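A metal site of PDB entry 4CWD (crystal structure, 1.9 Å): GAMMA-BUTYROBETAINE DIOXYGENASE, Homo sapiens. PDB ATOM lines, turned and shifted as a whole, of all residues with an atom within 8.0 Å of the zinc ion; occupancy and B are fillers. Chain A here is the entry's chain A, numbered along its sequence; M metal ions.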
ATOM      1  N   LEU A  35      21.754 -25.194  -8.582  1.00  0.00           N
ATOM      2  CA  LEU A  35      23.066 -24.585  -8.408  1.00  0.00           C
ATOM      3  C   LEU A  35      23.515 -23.900  -9.688  1.00  0.00           C
ATOM      4  O   LEU A  35      23.962 -22.742  -9.657  1.00  0.00           O
ATOM      5  CB  LEU A  35      24.096 -25.645  -7.993  1.00  0.00           C
ATOM      6  CG  LEU A  35      23.863 -26.216  -6.587  1.00  0.00           C
ATOM      7  CD1 LEU A  35      24.701 -27.474  -6.358  1.00  0.00           C
ATOM      8  CD2 LEU A  35      24.155 -25.172  -5.508  1.00  0.00           C
ATOM      9  N   ARG A  36      23.388 -24.574 -10.815  1.00  0.00           N
ATOM     10  CA  ARG A  36      23.859 -23.999 -12.073  1.00  0.00           C
ATOM     11  C   ARG A  36      23.046 -22.754 -12.422  1.00  0.00           C
ATOM     12  O   ARG A  36      23.601 -21.733 -12.827  1.00  0.00           O
ATOM     13  CB  ARG A  36      23.791 -25.020 -13.211  1.00  0.00           C
ATOM     14  CG  ARG A  36      24.210 -24.462 -14.562  1.00  0.00           C
ATOM     15  CD  ARG A  36      25.712 -24.124 -14.564  1.00  0.00           C
ATOM     16  NE  ARG A  36      26.134 -23.434 -15.783  1.00  0.00           N
ATOM     17  CZ  ARG A  36      26.102 -22.112 -15.950  1.00  0.00           C
ATOM     18  NH1 ARG A  36      25.620 -21.325 -14.989  1.00  0.00           N
ATOM     19  NH2 ARG A  36      26.530 -21.572 -17.089  1.00  0.00           N
ATOM     20  N   ASP A  37      21.727 -22.873 -12.253  1.00  0.00           N
ATOM     21  CA  ASP A  37      20.793 -21.767 -12.478  1.00  0.00           C
ATOM     22  C   ASP A  37      21.175 -20.515 -11.674  1.00  0.00           C
ATOM     23  O   ASP A  37      20.934 -19.386 -12.109  1.00  0.00           O
ATOM     24  CB  ASP A  37      19.367 -22.189 -12.090  1.00  0.00           C
ATOM     25  CG  ASP A  37      18.341 -21.099 -12.331  1.00  0.00           C
ATOM     26  OD1 ASP A  37      18.289 -20.576 -13.445  1.00  0.00           O
ATOM     27  OD2 ASP A  37      17.558 -20.786 -11.397  1.00  0.00           O
ATOM     28  N   ASN A  38      21.774 -20.727 -10.524  1.00  0.00           N
ATOM     29  CA  ASN A  38      22.037 -19.642  -9.583  1.00  0.00           C
ATOM     30  C   ASN A  38      23.517 -19.389  -9.346  1.00  0.00           C
ATOM     31  O   ASN A  38      23.918 -18.822  -8.324  1.00  0.00           O
ATOM     32  CB  ASN A  38      21.286 -19.930  -8.284  1.00  0.00           C
ATOM     33  CG  ASN A  38      19.812 -19.719  -8.442  1.00  0.00           C
ATOM     34  OD1 ASN A  38      19.386 -18.640  -8.812  1.00  0.00           O
ATOM     35  ND2 ASN A  38      19.011 -20.765  -8.228  1.00  0.00           N
ATOM     36  N   CYS A  39      24.325 -19.770 -10.333  1.00  0.00           N
ATOM     37  CA  CYS A  39      25.740 -19.404 -10.332  1.00  0.00           C
ATOM     38  C   CYS A  39      25.870 -17.900 -10.155  1.00  0.00           C
ATOM     39  O   CYS A  39      25.241 -17.149 -10.884  1.00  0.00           O
ATOM     40  CB  CYS A  39      26.393 -19.854 -11.639  1.00  0.00           C
ATOM     41  SG  CYS A  39      28.117 -19.327 -11.796  1.00  0.00           S
ATOM     42  N   PRO A  40      26.660 -17.436  -9.162  1.00  0.00           N
ATOM     43  CA  PRO A  40      26.802 -15.988  -8.965  1.00  0.00           C
ATOM     44  C   PRO A  40      27.972 -15.329  -9.738  1.00  0.00           C
ATOM     45  O   PRO A  40      28.300 -14.178  -9.451  1.00  0.00           O
ATOM     46  CB  PRO A  40      27.037 -15.876  -7.454  1.00  0.00           C
ATOM     47  CG  PRO A  40      27.793 -17.122  -7.120  1.00  0.00           C
ATOM     48  CD  PRO A  40      27.281 -18.201  -8.072  1.00  0.00           C
ATOM     49  N   CYS A  41      28.588 -16.007 -10.705  1.00  0.00           N
ATOM     50  CA  CYS A  41      29.707 -15.408 -11.432  1.00  0.00           C
ATOM     51  C   CYS A  41      29.196 -14.301 -12.343  1.00  0.00           C
ATOM     52  O   CYS A  41      27.997 -14.227 -12.623  1.00  0.00           O
ATOM     53  CB  CYS A  41      30.467 -16.458 -12.249  1.00  0.00           C
ATOM     54  SG  CYS A  41      29.839 -16.717 -13.925  1.00  0.00           S
ATOM     55  N   SER A  42      30.101 -13.460 -12.834  1.00  0.00           N
ATOM     56  CA  SER A  42      29.690 -12.261 -13.555  1.00  0.00           C
ATOM     57  C   SER A  42      29.068 -12.558 -14.920  1.00  0.00           C
ATOM     58  O   SER A  42      28.381 -11.706 -15.479  1.00  0.00           O
ATOM     59  CB  SER A  42      30.875 -11.312 -13.713  1.00  0.00           C
ATOM     60  OG  SER A  42      31.936 -11.931 -14.410  1.00  0.00           O
ATOM     61  N   ASP A  43      29.287 -13.756 -15.468  1.00  0.00           N
ATOM     62  CA  ASP A  43      28.591 -14.147 -16.693  1.00  0.00           C
ATOM     63  C   ASP A  43      27.106 -14.393 -16.438  1.00  0.00           C
ATOM     64  O   ASP A  43      26.270 -14.112 -17.291  1.00  0.00           O
ATOM     65  CB  ASP A  43      29.174 -15.415 -17.309  1.00  0.00           C
ATOM     66  CG  ASP A  43      30.583 -15.229 -17.834  1.00  0.00           C
ATOM     67  OD1 ASP A  43      31.086 -14.091 -17.856  1.00  0.00           O
ATOM     68  OD2 ASP A  43      31.163 -16.252 -18.247  1.00  0.00           O
ATOM     69  N   CYS A  44      26.801 -14.952 -15.267  1.00  0.00           N
ATOM     70  CA  CYS A  44      25.479 -15.501 -14.974  1.00  0.00           C
ATOM     71  C   CYS A  44      24.608 -14.579 -14.149  1.00  0.00           C
ATOM     72  O   CYS A  44      23.387 -14.747 -14.097  1.00  0.00           O
ATOM     73  CB  CYS A  44      25.603 -16.830 -14.221  1.00  0.00           C
ATOM     74  SG  CYS A  44      26.468 -18.107 -15.108  1.00  0.00           S
ATOM     75  N   TYR A  45      25.244 -13.599 -13.511  1.00  0.00           N
ATOM     76  CA  TYR A  45      24.594 -12.811 -12.471  1.00  0.00           C
ATOM     77  C   TYR A  45      25.092 -11.377 -12.480  1.00  0.00           C
ATOM     78  O   TYR A  45      26.297 -11.143 -12.438  1.00  0.00           O
ATOM     79  CB  TYR A  45      24.875 -13.441 -11.116  1.00  0.00           C
ATOM     80  CG  TYR A  45      24.010 -12.890 -10.000  1.00  0.00           C
ATOM     81  CD1 TYR A  45      22.739 -13.388  -9.794  1.00  0.00           C
ATOM     82  CD2 TYR A  45      24.465 -11.877  -9.173  1.00  0.00           C
ATOM     83  CE1 TYR A  45      21.939 -12.904  -8.779  1.00  0.00           C
ATOM     84  CE2 TYR A  45      23.658 -11.375  -8.143  1.00  0.00           C
ATOM     85  CZ  TYR A  45      22.402 -11.894  -7.959  1.00  0.00           C
ATOM     86  OH  TYR A  45      21.574 -11.417  -6.956  1.00  0.00           O
ATOM     87  N   LEU A  54      21.789 -15.241 -16.610  1.00  0.00           N
ATOM     88  CA  LEU A  54      21.674 -16.557 -17.225  1.00  0.00           C
ATOM     89  C   LEU A  54      20.293 -16.780 -17.808  1.00  0.00           C
ATOM     90  O   LEU A  54      19.289 -16.493 -17.161  1.00  0.00           O
ATOM     91  CB  LEU A  54      21.967 -17.650 -16.202  1.00  0.00           C
ATOM     92  CG  LEU A  54      22.082 -19.085 -16.736  1.00  0.00           C
ATOM     93  CD1 LEU A  54      23.387 -19.251 -17.506  1.00  0.00           C
ATOM     94  CD2 LEU A  54      21.985 -20.101 -15.601  1.00  0.00           C
ATOM     95  N   TRP A  79      31.408 -27.531 -14.049  1.00  0.00           N
ATOM     96  CA  TRP A  79      30.311 -28.139 -14.782  1.00  0.00           C
ATOM     97  C   TRP A  79      30.813 -28.856 -16.038  1.00  0.00           C
ATOM     98  O   TRP A  79      31.938 -28.625 -16.490  1.00  0.00           O
ATOM     99  CB  TRP A  79      29.284 -27.087 -15.147  1.00  0.00           C
ATOM    100  CG  TRP A  79      28.718 -26.397 -13.934  1.00  0.00           C
ATOM    101  CD1 TRP A  79      29.038 -25.160 -13.492  1.00  0.00           C
ATOM    102  CD2 TRP A  79      27.756 -26.925 -13.021  1.00  0.00           C
ATOM    103  NE1 TRP A  79      28.327 -24.864 -12.354  1.00  0.00           N
ATOM    104  CE2 TRP A  79      27.538 -25.938 -12.040  1.00  0.00           C
ATOM    105  CE3 TRP A  79      27.069 -28.131 -12.926  1.00  0.00           C
ATOM    106  CZ2 TRP A  79      26.636 -26.125 -10.987  1.00  0.00           C
ATOM    107  CZ3 TRP A  79      26.173 -28.312 -11.885  1.00  0.00           C
ATOM    108  CH2 TRP A  79      25.975 -27.315 -10.932  1.00  0.00           C
ATOM    109  N   HIS A  83      32.019 -24.655 -17.426  1.00  0.00           N
ATOM    110  CA  HIS A  83      31.656 -23.508 -16.617  1.00  0.00           C
ATOM    111  C   HIS A  83      32.071 -23.771 -15.174  1.00  0.00           C
ATOM    112  O   HIS A  83      32.157 -24.933 -14.755  1.00  0.00           O
ATOM    113  CB  HIS A  83      30.158 -23.201 -16.688  1.00  0.00           C
ATOM    114  CG  HIS A  83      29.817 -21.818 -16.222  1.00  0.00           C
ATOM    115  ND1 HIS A  83      29.998 -20.707 -17.018  1.00  0.00           N
ATOM    116  CD2 HIS A  83      29.330 -21.361 -15.044  1.00  0.00           C
ATOM    117  CE1 HIS A  83      29.621 -19.630 -16.348  1.00  0.00           C
ATOM    118  NE2 HIS A  83      29.227 -20.004 -15.150  1.00  0.00           N
ATOM    119  N   TYR A  84      32.350 -22.715 -14.431  1.00  0.00           N
ATOM    120  CA  TYR A  84      32.887 -22.835 -13.082  1.00  0.00           C
ATOM    121  C   TYR A  84      32.106 -21.930 -12.123  1.00  0.00           C
ATOM    122  O   TYR A  84      31.838 -20.762 -12.450  1.00  0.00           O
ATOM    123  CB  TYR A  84      34.367 -22.495 -13.076  1.00  0.00           C
ATOM    124  CG  TYR A  84      34.961 -22.312 -11.710  1.00  0.00           C
ATOM    125  CD1 TYR A  84      35.240 -23.394 -10.889  1.00  0.00           C
ATOM    126  CD2 TYR A  84      35.239 -21.044 -11.220  1.00  0.00           C
ATOM    127  CE1 TYR A  84      35.775 -23.222  -9.627  1.00  0.00           C
ATOM    128  CE2 TYR A  84      35.780 -20.860  -9.957  1.00  0.00           C
ATOM    129  CZ  TYR A  84      36.052 -21.958  -9.168  1.00  0.00           C
ATOM    130  OH  TYR A  84      36.594 -21.789  -7.912  1.00  0.00           O
ATOM    131  N   SER A  85      31.735 -22.468 -10.969  1.00  0.00           N
ATOM    132  CA  SER A  85      30.904 -21.748  -9.991  1.00  0.00           C
ATOM    133  C   SER A  85      31.453 -21.814  -8.558  1.00  0.00           C
ATOM    134  O   SER A  85      32.018 -22.831  -8.155  1.00  0.00           O
ATOM    135  CB  SER A  85      29.480 -22.292  -9.991  1.00  0.00           C
ATOM    136  OG  SER A  85      28.901 -22.247 -11.281  1.00  0.00           O
ATOM    137  N   GLU A  86      31.257 -20.736  -7.802  1.00  0.00           N
ATOM    138  CA  GLU A  86      31.573 -20.716  -6.379  1.00  0.00           C
ATOM    139  C   GLU A  86      30.331 -20.304  -5.596  1.00  0.00           C
ATOM    140  O   GLU A  86      29.664 -19.345  -5.962  1.00  0.00           O
ATOM    141  CB  GLU A  86      32.724 -19.766  -6.074  1.00  0.00           C
ATOM    142  CG  GLU A  86      34.022 -20.112  -6.779  1.00  0.00           C
ATOM    143  CD  GLU A  86      35.180 -19.217  -6.383  1.00  0.00           C
ATOM    144  OE1 GLU A  86      34.957 -18.264  -5.605  1.00  0.00           O
ATOM    145  OE2 GLU A  86      36.315 -19.460  -6.847  1.00  0.00           O
ATOM    146  N   PHE A  87      30.041 -21.032  -4.523  1.00  0.00           N
ATOM    147  CA  PHE A  87      28.895 -20.751  -3.660  1.00  0.00           C
ATOM    148  C   PHE A  87      29.354 -20.616  -2.207  1.00  0.00           C
ATOM    149  O   PHE A  87      30.142 -21.435  -1.736  1.00  0.00           O
ATOM    150  CB  PHE A  87      27.854 -21.870  -3.781  1.00  0.00           C
ATOM    151  CG  PHE A  87      27.361 -22.101  -5.171  1.00  0.00           C
ATOM    152  CD1 PHE A  87      26.269 -21.405  -5.660  1.00  0.00           C
ATOM    153  CD2 PHE A  87      27.997 -23.005  -6.012  1.00  0.00           C
ATOM    154  CE1 PHE A  87      25.820 -21.599  -6.959  1.00  0.00           C
ATOM    155  CE2 PHE A  87      27.556 -23.210  -7.313  1.00  0.00           C
ATOM    156  CZ  PHE A  87      26.470 -22.505  -7.783  1.00  0.00           C
HETATM  157 ZN    ZN M   1      28.358 -18.589 -13.866  1.00  0.00          ZN
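SG of Cys 39 lies close to OG of Ser 85. The side-chain sulfur of Cys 44 sits close to the guanidinium group of Arg 36 (3.3 Å). The backbone carbonyl oxygen (O) of Cys 44 lies within hydrogen-bond range of the backbone NH (N) of Leu 54 (3.0 Å). The side-chain sulfur of Cys 41 sits close to the backbone NH of Asp 43, at 3.4 Å.
Four residues have an atom within 4 Å of the zinc ion: Cys 39, Cys 41, Cys 44 and His 83.
The zinc ion is bound by a ring nitrogen (NE2) of His 83 (2.1 Å), the side-chain sulfur (SG) of Cys 39 (2.2 Å), the side-chain sulfur (SG) of Cys 44 (2.3 Å) and the side-chain sulfur (SG) of Cys 41 (2.4 Å).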
